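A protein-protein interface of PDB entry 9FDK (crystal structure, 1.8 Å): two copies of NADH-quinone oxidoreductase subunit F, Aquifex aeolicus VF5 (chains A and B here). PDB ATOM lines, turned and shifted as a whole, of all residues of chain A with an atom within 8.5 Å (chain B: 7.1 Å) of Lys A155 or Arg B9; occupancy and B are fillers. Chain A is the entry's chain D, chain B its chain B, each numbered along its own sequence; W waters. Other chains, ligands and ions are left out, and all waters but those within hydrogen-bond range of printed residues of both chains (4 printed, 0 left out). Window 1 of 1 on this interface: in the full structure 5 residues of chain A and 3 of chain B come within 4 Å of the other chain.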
ATOM      1  N   SER A  30       8.455  -3.710 -35.209  1.00  0.00           N
ATOM      2  CA  SER A  30       8.949  -3.469 -33.862  1.00  0.00           C
ATOM      3  C   SER A  30       9.174  -1.972 -33.655  1.00  0.00           C
ATOM      4  O   SER A  30       8.855  -1.162 -34.524  1.00  0.00           O
ATOM      5  CB  SER A  30      10.158  -4.339 -33.599  1.00  0.00           C
ATOM      6  OG  SER A  30       9.738  -5.701 -33.513  1.00  0.00           O
ATOM      7  N   ILE A  31       9.686  -1.590 -32.483  1.00  0.00           N
ATOM      8  CA  ILE A  31       9.604  -0.204 -32.064  1.00  0.00           C
ATOM      9  C   ILE A  31      10.424   0.711 -32.978  1.00  0.00           C
ATOM     10  O   ILE A  31      10.022   1.848 -33.215  1.00  0.00           O
ATOM     11  CB  ILE A  31       9.962  -0.063 -30.570  1.00  0.00           C
ATOM     12  CG1 ILE A  31       9.374   1.234 -30.000  1.00  0.00           C
ATOM     13  CG2 ILE A  31      11.463  -0.178 -30.327  1.00  0.00           C
ATOM     14  CD1 ILE A  31       9.367   1.305 -28.484  1.00  0.00           C
ATOM     15  N   ASP A  32      11.561   0.238 -33.495  1.00  0.00           N
ATOM     16  CA  ASP A  32      12.402   1.085 -34.331  1.00  0.00           C
ATOM     17  C   ASP A  32      11.668   1.495 -35.607  1.00  0.00           C
ATOM     18  O   ASP A  32      11.680   2.668 -35.977  1.00  0.00           O
ATOM     19  CB  ASP A  32      13.742   0.440 -34.627  1.00  0.00           C
ATOM     20  CG  ASP A  32      14.740   0.429 -33.474  1.00  0.00           C
ATOM     21  OD1 ASP A  32      14.575   1.193 -32.487  1.00  0.00           O
ATOM     22  OD2 ASP A  32      15.694  -0.351 -33.574  1.00  0.00           O
ATOM     23  N   LEU A  35       8.991   4.006 -34.610  1.00  0.00           N
ATOM     24  CA  LEU A  35       9.563   5.321 -34.336  1.00  0.00           C
ATOM     25  C   LEU A  35       9.928   6.061 -35.628  1.00  0.00           C
ATOM     26  O   LEU A  35       9.750   7.272 -35.727  1.00  0.00           O
ATOM     27  CB  LEU A  35      10.775   5.130 -33.425  1.00  0.00           C
ATOM     28  CG  LEU A  35      10.460   4.772 -31.968  1.00  0.00           C
ATOM     29  CD1 LEU A  35      11.708   4.308 -31.228  1.00  0.00           C
ATOM     30  CD2 LEU A  35       9.868   5.961 -31.244  1.00  0.00           C
ATOM     31  N   GLY A  39       6.143   7.370 -34.651  1.00  0.00           N
ATOM     32  CA  GLY A  39       5.454   6.745 -33.542  1.00  0.00           C
ATOM     33  C   GLY A  39       5.912   7.325 -32.208  1.00  0.00           C
ATOM     34  O   GLY A  39       7.071   7.703 -32.051  1.00  0.00           O
ATOM     35  N   TYR A  40       4.968   7.380 -31.261  1.00  0.00           N
ATOM     36  CA  TYR A  40       5.184   7.848 -29.902  1.00  0.00           C
ATOM     37  C   TYR A  40       5.351   9.368 -29.843  1.00  0.00           C
ATOM     38  O   TYR A  40       5.451   9.915 -28.756  1.00  0.00           O
ATOM     39  CB  TYR A  40       6.333   7.100 -29.214  1.00  0.00           C
ATOM     40  CG  TYR A  40       5.927   5.692 -28.804  1.00  0.00           C
ATOM     41  CD1 TYR A  40       4.972   5.485 -27.810  1.00  0.00           C
ATOM     42  CD2 TYR A  40       6.483   4.574 -29.407  1.00  0.00           C
ATOM     43  CE1 TYR A  40       4.598   4.211 -27.430  1.00  0.00           C
ATOM     44  CE2 TYR A  40       6.095   3.292 -29.055  1.00  0.00           C
ATOM     45  CZ  TYR A  40       5.164   3.111 -28.052  1.00  0.00           C
ATOM     46  OH  TYR A  40       4.782   1.857 -27.694  1.00  0.00           O
ATOM     47  N   LEU A  43       2.072  10.536 -28.240  1.00  0.00           N
ATOM     48  CA  LEU A  43       2.202  10.417 -26.800  1.00  0.00           C
ATOM     49  C   LEU A  43       2.902  11.644 -26.232  1.00  0.00           C
ATOM     50  O   LEU A  43       2.440  12.199 -25.247  1.00  0.00           O
ATOM     51  CB  LEU A  43       2.954   9.157 -26.392  1.00  0.00           C
ATOM     52  CG  LEU A  43       3.218   9.013 -24.889  1.00  0.00           C
ATOM     53  CD1 LEU A  43       1.919   9.039 -24.084  1.00  0.00           C
ATOM     54  CD2 LEU A  43       3.990   7.738 -24.605  1.00  0.00           C
ATOM     55  N   GLU A  44       4.044  12.041 -26.813  1.00  0.00           N
ATOM     56  CA  GLU A  44       4.793  13.175 -26.276  1.00  0.00           C
ATOM     57  C   GLU A  44       3.926  14.434 -26.257  1.00  0.00           C
ATOM     58  O   GLU A  44       3.959  15.203 -25.303  1.00  0.00           O
ATOM     59  CB  GLU A  44       6.062  13.443 -27.080  1.00  0.00           C
ATOM     60  CG  GLU A  44       7.119  12.356 -26.934  1.00  0.00           C
ATOM     61  CD  GLU A  44       8.310  12.631 -27.834  1.00  0.00           C
ATOM     62  OE1 GLU A  44       8.267  12.265 -29.014  1.00  0.00           O
ATOM     63  OE2 GLU A  44       9.256  13.276 -27.364  1.00  0.00           O
ATOM     64  N   HIS A 112       2.688  -1.391 -31.330  1.00  0.00           N
ATOM     65  CA  HIS A 112       3.015  -0.112 -30.713  1.00  0.00           C
ATOM     66  C   HIS A 112       1.919   0.926 -30.952  1.00  0.00           C
ATOM     67  O   HIS A 112       1.778   1.832 -30.137  1.00  0.00           O
ATOM     68  CB  HIS A 112       4.396   0.389 -31.135  1.00  0.00           C
ATOM     69  CG  HIS A 112       5.464  -0.437 -30.526  1.00  0.00           C
ATOM     70  ND1 HIS A 112       5.776  -0.334 -29.186  1.00  0.00           N
ATOM     71  CD2 HIS A 112       6.238  -1.406 -31.031  1.00  0.00           C
ATOM     72  CE1 HIS A 112       6.715  -1.222 -28.908  1.00  0.00           C
ATOM     73  NE2 HIS A 112       7.033  -1.870 -30.018  1.00  0.00           N
ATOM     74  N   ALA A 148       6.518  -6.185 -27.075  1.00  0.00           N
ATOM     75  CA  ALA A 148       6.386  -4.782 -27.435  1.00  0.00           C
ATOM     76  C   ALA A 148       6.313  -3.919 -26.173  1.00  0.00           C
ATOM     77  O   ALA A 148       6.912  -2.846 -26.119  1.00  0.00           O
ATOM     78  CB  ALA A 148       5.187  -4.571 -28.328  1.00  0.00           C
ATOM     79  N   ILE A 149       5.615  -4.397 -25.140  1.00  0.00           N
ATOM     80  CA  ILE A 149       5.555  -3.658 -23.884  1.00  0.00           C
ATOM     81  C   ILE A 149       6.967  -3.467 -23.322  1.00  0.00           C
ATOM     82  O   ILE A 149       7.329  -2.370 -22.880  1.00  0.00           O
ATOM     83  CB  ILE A 149       4.574  -4.336 -22.910  1.00  0.00           C
ATOM     84  CG1 ILE A 149       3.141  -4.010 -23.318  1.00  0.00           C
ATOM     85  CG2 ILE A 149       4.855  -3.958 -21.451  1.00  0.00           C
ATOM     86  CD1 ILE A 149       2.092  -4.918 -22.717  1.00  0.00           C
ATOM     87  N   GLU A 150       7.781  -4.524 -23.348  1.00  0.00           N
ATOM     88  CA  GLU A 150       9.146  -4.417 -22.857  1.00  0.00           C
ATOM     89  C   GLU A 150       9.935  -3.409 -23.694  1.00  0.00           C
ATOM     90  O   GLU A 150      10.720  -2.639 -23.135  1.00  0.00           O
ATOM     91  CB  GLU A 150       9.879  -5.760 -22.822  1.00  0.00           C
ATOM     92  CG  GLU A 150       9.327  -6.735 -21.786  1.00  0.00           C
ATOM     93  CD  GLU A 150       9.190  -6.163 -20.377  1.00  0.00           C
ATOM     94  OE1 GLU A 150      10.192  -5.590 -19.898  1.00  0.00           O
ATOM     95  OE2 GLU A 150       8.080  -6.269 -19.778  1.00  0.00           O
ATOM     96  N   GLU A 151       9.760  -3.434 -25.026  1.00  0.00           N
ATOM     97  CA  GLU A 151      10.391  -2.439 -25.888  1.00  0.00           C
ATOM     98  C   GLU A 151      10.008  -1.019 -25.444  1.00  0.00           C
ATOM     99  O   GLU A 151      10.861  -0.130 -25.369  1.00  0.00           O
ATOM    100  CB  GLU A 151      10.026  -2.566 -27.371  1.00  0.00           C
ATOM    101  CG  GLU A 151      10.607  -3.770 -28.104  1.00  0.00           C
ATOM    102  CD  GLU A 151      10.190  -3.773 -29.585  1.00  0.00           C
ATOM    103  OE1 GLU A 151       8.989  -3.910 -29.942  1.00  0.00           O
ATOM    104  OE2 GLU A 151      11.101  -3.567 -30.413  1.00  0.00           O
ATOM    105  N   ALA A 152       8.718  -0.794 -25.197  1.00  0.00           N
ATOM    106  CA  ALA A 152       8.225   0.513 -24.797  1.00  0.00           C
ATOM    107  C   ALA A 152       8.846   0.922 -23.454  1.00  0.00           C
ATOM    108  O   ALA A 152       9.219   2.085 -23.268  1.00  0.00           O
ATOM    109  CB  ALA A 152       6.711   0.517 -24.745  1.00  0.00           C
ATOM    110  N   LYS A 153       8.978  -0.039 -22.529  1.00  0.00           N
ATOM    111  CA  LYS A 153       9.615   0.223 -21.242  1.00  0.00           C
ATOM    112  C   LYS A 153      11.062   0.680 -21.442  1.00  0.00           C
ATOM    113  O   LYS A 153      11.502   1.650 -20.835  1.00  0.00           O
ATOM    114  CB  LYS A 153       9.579  -1.005 -20.321  1.00  0.00           C
ATOM    115  CG  LYS A 153       8.185  -1.466 -19.872  1.00  0.00           C
ATOM    116  CD  LYS A 153       8.140  -2.498 -18.745  1.00  0.00           C
ATOM    117  CE  LYS A 153       8.613  -1.916 -17.443  1.00  0.00           C
ATOM    118  NZ  LYS A 153       8.349  -2.769 -16.278  1.00  0.00           N
ATOM    119  N   LYS A 154      11.798  -0.007 -22.322  1.00  0.00           N
ATOM    120  CA  LYS A 154      13.199   0.307 -22.570  1.00  0.00           C
ATOM    121  C   LYS A 154      13.373   1.718 -23.137  1.00  0.00           C
ATOM    122  O   LYS A 154      14.370   2.377 -22.844  1.00  0.00           O
ATOM    123  CB  LYS A 154      13.818  -0.771 -23.464  1.00  0.00           C
ATOM    124  CG  LYS A 154      13.916  -2.136 -22.761  1.00  0.00           C
ATOM    125  CD  LYS A 154      14.282  -3.342 -23.625  1.00  0.00           C
ATOM    126  CE  LYS A 154      14.193  -4.601 -22.809  1.00  0.00           C
ATOM    127  NZ  LYS A 154      14.732  -5.732 -23.561  1.00  0.00           N
ATOM    128  N   LYS A 155      12.388   2.199 -23.904  1.00  0.00           N
ATOM    129  CA  LYS A 155      12.462   3.514 -24.519  1.00  0.00           C
ATOM    130  C   LYS A 155      11.801   4.568 -23.633  1.00  0.00           C
ATOM    131  O   LYS A 155      11.673   5.715 -24.051  1.00  0.00           O
ATOM    132  CB  LYS A 155      11.791   3.505 -25.898  1.00  0.00           C
ATOM    133  CG  LYS A 155      12.456   2.599 -26.935  1.00  0.00           C
ATOM    134  CD  LYS A 155      13.808   3.099 -27.395  1.00  0.00           C
ATOM    135  CE  LYS A 155      14.344   2.420 -28.621  1.00  0.00           C
ATOM    136  NZ  LYS A 155      15.637   3.039 -28.942  1.00  0.00           N
ATOM    137  N   GLY A 156      11.319   4.163 -22.450  1.00  0.00           N
ATOM    138  CA  GLY A 156      10.812   5.103 -21.464  1.00  0.00           C
ATOM    139  C   GLY A 156       9.396   5.599 -21.752  1.00  0.00           C
ATOM    140  O   GLY A 156       9.004   6.632 -21.232  1.00  0.00           O
ATOM    141  N   PHE A 157       8.600   4.849 -22.534  1.00  0.00           N
ATOM    142  CA  PHE A 157       7.205   5.196 -22.763  1.00  0.00           C
ATOM    143  C   PHE A 157       6.268   4.584 -21.717  1.00  0.00           C
ATOM    144  O   PHE A 157       5.095   4.945 -21.685  1.00  0.00           O
ATOM    145  CB  PHE A 157       6.856   4.744 -24.182  1.00  0.00           C
ATOM    146  CG  PHE A 157       7.676   5.435 -25.263  1.00  0.00           C
ATOM    147  CD1 PHE A 157       7.838   6.820 -25.274  1.00  0.00           C
ATOM    148  CD2 PHE A 157       8.305   4.701 -26.260  1.00  0.00           C
ATOM    149  CE1 PHE A 157       8.582   7.447 -26.260  1.00  0.00           C
ATOM    150  CE2 PHE A 157       9.055   5.337 -27.240  1.00  0.00           C
ATOM    151  CZ  PHE A 157       9.199   6.705 -27.235  1.00  0.00           C
ATOM    152  N   LEU A 158       6.776   3.646 -20.903  1.00  0.00           N
ATOM    153  CA  LEU A 158       6.035   3.017 -19.816  1.00  0.00           C
ATOM    154  C   LEU A 158       6.916   3.034 -18.583  1.00  0.00           C
ATOM    155  O   LEU A 158       8.137   3.093 -18.708  1.00  0.00           O
ATOM    156  CB  LEU A 158       5.657   1.564 -20.118  1.00  0.00           C
ATOM    157  CG  LEU A 158       4.489   1.350 -21.076  1.00  0.00           C
ATOM    158  CD1 LEU A 158       4.355  -0.129 -21.405  1.00  0.00           C
ATOM    159  CD2 LEU A 158       3.219   1.896 -20.468  1.00  0.00           C
ATOM    160  N   GLY A 159       6.285   2.927 -17.410  1.00  0.00           N
ATOM    161  CA  GLY A 159       6.995   2.969 -16.138  1.00  0.00           C
ATOM    162  C   GLY A 159       6.553   4.174 -15.321  1.00  0.00           C
ATOM    163  O   GLY A 159       5.474   4.714 -15.544  1.00  0.00           O
ATOM    164  N   ASN A 161       6.832   8.097 -14.077  1.00  0.00           N
ATOM    165  CA  ASN A 161       7.291   9.415 -14.475  1.00  0.00           C
ATOM    166  C   ASN A 161       7.654   9.405 -15.956  1.00  0.00           C
ATOM    167  O   ASN A 161       8.765   9.778 -16.333  1.00  0.00           O
ATOM    168  CB  ASN A 161       8.457   9.850 -13.591  1.00  0.00           C
ATOM    169  CG  ASN A 161       8.932  11.245 -13.913  1.00  0.00           C
ATOM    170  OD1 ASN A 161       8.166  12.078 -14.417  1.00  0.00           O
ATOM    171  ND2 ASN A 161      10.193  11.519 -13.623  1.00  0.00           N
ATOM    172  N   ILE A 162       6.690   8.994 -16.788  1.00  0.00           N
ATOM    173  CA  ILE A 162       6.923   8.786 -18.206  1.00  0.00           C
ATOM    174  C   ILE A 162       7.311  10.114 -18.857  1.00  0.00           C
ATOM    175  O   ILE A 162       6.553  11.088 -18.817  1.00  0.00           O
ATOM    176  CB  ILE A 162       5.695   8.142 -18.870  1.00  0.00           C
ATOM    177  CG1 ILE A 162       5.448   6.734 -18.336  1.00  0.00           C
ATOM    178  CG2 ILE A 162       5.838   8.148 -20.388  1.00  0.00           C
ATOM    179  CD1 ILE A 162       4.047   6.196 -18.596  1.00  0.00           C
ATOM    180  N   LEU A 163       8.523  10.120 -19.440  1.00  0.00           N
ATOM    181  CA  LEU A 163       9.100  11.275 -20.119  1.00  0.00           C
ATOM    182  C   LEU A 163       8.990  12.541 -19.269  1.00  0.00           C
ATOM    183  O   LEU A 163       8.791  13.630 -19.795  1.00  0.00           O
ATOM    184  CB  LEU A 163       8.402  11.437 -21.466  1.00  0.00           C
ATOM    185  CG  LEU A 163       8.477  10.233 -22.409  1.00  0.00           C
ATOM    186  CD1 LEU A 163       7.687  10.520 -23.673  1.00  0.00           C
ATOM    187  CD2 LEU A 163       9.924   9.874 -22.741  1.00  0.00           C
ATOM    188  N   GLY A 164       9.163  12.405 -17.952  1.00  0.00           N
ATOM    189  CA  GLY A 164       9.241  13.558 -17.067  1.00  0.00           C
ATOM    190  C   GLY A 164       7.882  14.191 -16.756  1.00  0.00           C
ATOM    191  O   GLY A 164       7.841  15.274 -16.178  1.00  0.00           O
ATOM    192  N   ALA B   6      15.417  17.056 -22.556  1.00  0.00           N
ATOM    193  CA  ALA B   6      15.261  15.738 -23.161  1.00  0.00           C
ATOM    194  C   ALA B   6      16.594  14.986 -23.230  1.00  0.00           C
ATOM    195  O   ALA B   6      17.635  15.564 -23.537  1.00  0.00           O
ATOM    196  CB  ALA B   6      14.636  15.873 -24.531  1.00  0.00           C
ATOM    197  N   ILE B   7      16.549  13.694 -22.886  1.00  0.00           N
ATOM    198  CA  ILE B   7      17.684  12.778 -22.924  1.00  0.00           C
ATOM    199  C   ILE B   7      17.233  11.517 -23.654  1.00  0.00           C
ATOM    200  O   ILE B   7      16.207  10.963 -23.273  1.00  0.00           O
ATOM    201  CB  ILE B   7      18.124  12.329 -21.518  1.00  0.00           C
ATOM    202  CG1 ILE B   7      18.409  13.459 -20.566  1.00  0.00           C
ATOM    203  CG2 ILE B   7      19.316  11.367 -21.601  1.00  0.00           C
ATOM    204  CD1 ILE B   7      18.436  12.988 -19.121  1.00  0.00           C
ATOM    205  N   PRO B   8      18.010  10.959 -24.613  1.00  0.00           N
ATOM    206  CA  PRO B   8      17.671   9.654 -25.181  1.00  0.00           C
ATOM    207  C   PRO B   8      17.703   8.582 -24.091  1.00  0.00           C
ATOM    208  O   PRO B   8      18.486   8.665 -23.154  1.00  0.00           O
ATOM    209  CB  PRO B   8      18.700   9.392 -26.278  1.00  0.00           C
ATOM    210  CG  PRO B   8      19.619  10.590 -26.276  1.00  0.00           C
ATOM    211  CD  PRO B   8      19.292  11.480 -25.097  1.00  0.00           C
ATOM    212  N   ARG B   9      16.833   7.574 -24.225  1.00  0.00           N
ATOM    213  CA  ARG B   9      16.715   6.531 -23.219  1.00  0.00           C
ATOM    214  C   ARG B   9      17.636   5.369 -23.583  1.00  0.00           C
ATOM    215  O   ARG B   9      17.233   4.418 -24.261  1.00  0.00           O
ATOM    216  CB  ARG B   9      15.250   6.093 -23.078  1.00  0.00           C
ATOM    217  CG  ARG B   9      14.449   6.937 -22.095  1.00  0.00           C
ATOM    218  CD  ARG B   9      14.106   8.312 -22.622  1.00  0.00           C
ATOM    219  NE  ARG B   9      13.296   8.137 -23.826  1.00  0.00           N
ATOM    220  CZ  ARG B   9      12.944   9.042 -24.736  1.00  0.00           C
ATOM    221  NH1 ARG B   9      12.069   8.683 -25.662  1.00  0.00           N
ATOM    222  NH2 ARG B   9      13.426  10.279 -24.705  1.00  0.00           N
ATOM    223  N   ILE B  10      18.889   5.487 -23.159  1.00  0.00           N
ATOM    224  CA  ILE B  10      19.915   4.481 -23.400  1.00  0.00           C
ATOM    225  C   ILE B  10      19.528   3.194 -22.680  1.00  0.00           C
ATOM    226  O   ILE B  10      19.169   3.234 -21.514  1.00  0.00           O
ATOM    227  CB  ILE B  10      21.271   5.031 -22.926  1.00  0.00           C
ATOM    228  CG1 ILE B  10      21.698   6.196 -23.800  1.00  0.00           C
ATOM    229  CG2 ILE B  10      22.352   3.942 -22.850  1.00  0.00           C
ATOM    230  CD1 ILE B  10      22.822   7.026 -23.225  1.00  0.00           C
ATOM    231  N   TYR B  11      19.602   2.059 -23.392  1.00  0.00           N
ATOM    232  CA  TYR B  11      19.330   0.761 -22.814  1.00  0.00           C
ATOM    233  C   TYR B  11      20.420   0.395 -21.804  1.00  0.00           C
ATOM    234  O   TYR B  11      21.605   0.580 -22.045  1.00  0.00           O
ATOM    235  CB  TYR B  11      19.178  -0.296 -23.914  1.00  0.00           C
ATOM    236  CG  TYR B  11      18.950  -1.686 -23.334  1.00  0.00           C
ATOM    237  CD1 TYR B  11      17.789  -1.973 -22.614  1.00  0.00           C
ATOM    238  CD2 TYR B  11      19.868  -2.710 -23.514  1.00  0.00           C
ATOM    239  CE1 TYR B  11      17.565  -3.227 -22.072  1.00  0.00           C
ATOM    240  CE2 TYR B  11      19.651  -3.976 -22.991  1.00  0.00           C
ATOM    241  CZ  TYR B  11      18.500  -4.234 -22.262  1.00  0.00           C
ATOM    242  OH  TYR B  11      18.264  -5.479 -21.742  1.00  0.00           O
ATOM    243  N   ALA B  12      19.997  -0.213 -20.692  1.00  0.00           N
ATOM    244  CA  ALA B  12      20.933  -0.675 -19.685  1.00  0.00           C
ATOM    245  C   ALA B  12      20.485  -2.024 -19.120  1.00  0.00           C
ATOM    246  O   ALA B  12      19.292  -2.262 -18.904  1.00  0.00           O
ATOM    247  CB  ALA B  12      21.075   0.387 -18.624  1.00  0.00           C
ATOM    248  N   PRO B  26      15.219   3.994 -17.103  1.00  0.00           N
ATOM    249  CA  PRO B  26      15.669   5.276 -17.659  1.00  0.00           C
ATOM    250  C   PRO B  26      14.917   6.519 -17.191  1.00  0.00           C
ATOM    251  O   PRO B  26      14.200   7.157 -17.958  1.00  0.00           O
ATOM    252  CB  PRO B  26      15.491   5.009 -19.153  1.00  0.00           C
ATOM    253  CG  PRO B  26      14.262   4.140 -19.230  1.00  0.00           C
ATOM    254  CD  PRO B  26      14.412   3.210 -18.049  1.00  0.00           C
ATOM    255  N   ARG B  27      15.126   6.868 -15.919  1.00  0.00           N
ATOM    256  CA  ARG B  27      14.505   8.041 -15.327  1.00  0.00           C
ATOM    257  C   ARG B  27      15.308   8.442 -14.093  1.00  0.00           C
ATOM    258  O   ARG B  27      16.087   7.639 -13.580  1.00  0.00           O
ATOM    259  CB  ARG B  27      13.056   7.749 -14.937  1.00  0.00           C
ATOM    260  CG  ARG B  27      12.895   6.607 -13.947  1.00  0.00           C
ATOM    261  CD  ARG B  27      11.448   6.289 -13.599  1.00  0.00           C
ATOM    262  NE  ARG B  27      11.342   5.226 -12.598  1.00  0.00           N
ATOM    263  CZ  ARG B  27      11.570   5.356 -11.291  1.00  0.00           C
ATOM    264  NH1 ARG B  27      11.462   4.315 -10.475  1.00  0.00           N
ATOM    265  NH2 ARG B  27      11.939   6.524 -10.798  1.00  0.00           N
ATOM    266  N   ILE B 105      24.665   7.538 -17.403  1.00  0.00           N
ATOM    267  CA  ILE B 105      23.427   6.928 -16.952  1.00  0.00           C
ATOM    268  C   ILE B 105      23.414   6.822 -15.426  1.00  0.00           C
ATOM    269  O   ILE B 105      22.333   6.846 -14.833  1.00  0.00           O
ATOM    270  CB  ILE B 105      23.112   5.586 -17.628  1.00  0.00           C
ATOM    271  CG1 ILE B 105      24.131   4.529 -17.269  1.00  0.00           C
ATOM    272  CG2 ILE B 105      22.932   5.739 -19.149  1.00  0.00           C
ATOM    273  CD1 ILE B 105      23.616   3.123 -17.491  1.00  0.00           C
ATOM    274  N   ARG B 109      20.399   9.051 -13.741  1.00  0.00           N
ATOM    275  CA  ARG B 109      19.352   8.164 -13.263  1.00  0.00           C
ATOM    276  C   ARG B 109      19.485   7.843 -11.784  1.00  0.00           C
ATOM    277  O   ARG B 109      18.474   7.614 -11.133  1.00  0.00           O
ATOM    278  CB  ARG B 109      19.321   6.838 -14.029  1.00  0.00           C
ATOM    279  CG  ARG B 109      19.057   7.048 -15.507  1.00  0.00           C
ATOM    280  CD  ARG B 109      19.295   5.776 -16.296  1.00  0.00           C
ATOM    281  NE  ARG B 109      19.188   6.046 -17.729  1.00  0.00           N
ATOM    282  CZ  ARG B 109      19.091   5.095 -18.664  1.00  0.00           C
ATOM    283  NH1 ARG B 109      19.146   3.806 -18.338  1.00  0.00           N
ATOM    284  NH2 ARG B 109      18.930   5.448 -19.925  1.00  0.00           N
ATOM    285  N   PRO B 261      22.372  -2.098 -28.544  1.00  0.00           N
ATOM    286  CA  PRO B 261      23.377  -1.161 -28.057  1.00  0.00           C
ATOM    287  C   PRO B 261      22.894  -0.600 -26.728  1.00  0.00           C
ATOM    288  O   PRO B 261      21.688  -0.444 -26.536  1.00  0.00           O
ATOM    289  CB  PRO B 261      23.484  -0.114 -29.177  1.00  0.00           C
ATOM    290  CG  PRO B 261      22.127  -0.157 -29.827  1.00  0.00           C
ATOM    291  CD  PRO B 261      21.693  -1.628 -29.762  1.00  0.00           C
HETATM  292  O   HOH W   1      11.574   9.443 -12.025  1.00  0.00           O
HETATM  293  O   HOH W   2      16.395   2.295 -21.132  1.00  0.00           O
HETATM  294  O   HOH W   3      12.541  12.726 -26.450  1.00  0.00           O
HETATM  295  O   HOH W   4      17.021   2.544 -26.205  1.00  0.00           O
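Arg B9 touches Lys A154 (O to O, 3.8 Å). Tyr B11 touches Lys A154 (CE1 to CD, 3.6 Å). Phe A157 touches Arg B9. Arg B9 touches Leu A163 (CZ to CD2, 3.7 Å).
Lys A155 touches just one residue of chain B: Arg B9 (2.9 Å). Arg B9 touches just these residues of chain A: Lys A154, Lys A155, Phe A157 and Leu A163. Of the printed residues of chain B, Leu A163 touches Arg B9 (3.7 Å). Printed residues of chain A within 4 Å of Tyr B11: Lys A154. Printed residues of chain B within 4 Å of Lys A154: Arg B9 and Tyr B11. Pro B26 touches none of the printed residues of chain A. Ala B6 touches none of the printed residues of chain A. The nearest residue of chain A that does not touch Arg B9 is Gly A156 (4.1 Å). The nearest printed residue of chain B that does not touch Lys A154 is Pro B26 (4.02 Å).
Of the 12 printed residues of chain B, 2 touch a printed residue of chain A. Hydrophobic or aromatic side chains of chain B that line the printed part of chain A: Tyr B11. Printed residues of chain A that touch a printed residue of chain B: Lys A154, Lys A155, Phe A157 and Leu A163. Hydrophobic or aromatic side chains of chain A that line the printed part of chain B: Phe A157 and Leu A163. Among the printed residues, 5 pairs touch across the chains. Among the printed residues, no Asp or Glu carboxylate lies within 4 Å of a Lys or Arg side-chain nitrogen of the other chain.
Water W2 lies within hydrogen-bond range of the backbone carbonyl oxygen (O) of Lys A154 (2.7 Å) and the backbone carbonyl oxygen (O) of Ile B10 (3.0 Å). Water W4 bridges the backbone carbonyl oxygen (O) of Arg B9 (2.7 Å) and the side-chain amino group (NZ) of Lys A155 (3.1 Å). Water W1 lies within hydrogen-bond range of the side-chain amide nitrogen (ND2) of Asn A161 and the guanidinium group (NH2) of Arg B27. Water W3 bridges the guanidinium group (NH2) of Arg B9 and the side-chain carboxylate (OE2) of Glu A44.
No position is printed for both chains. Of the 5 pairs that touch across the chains among the printed residues, none has its exchanged pair printed and touching as well.
NE of Arg B9 sits at hydrogen-bond distance from O of Lys A155, 2.9 Å away.
The guanidinium group (NH2) of Arg B9 is in hydrogen-bond range of the backbone carbonyl oxygen (O) of Ile B7 (3.2 Å). O of Ala A152 lies within hydrogen-bond range of N of Phe A157, at 2.9 Å.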
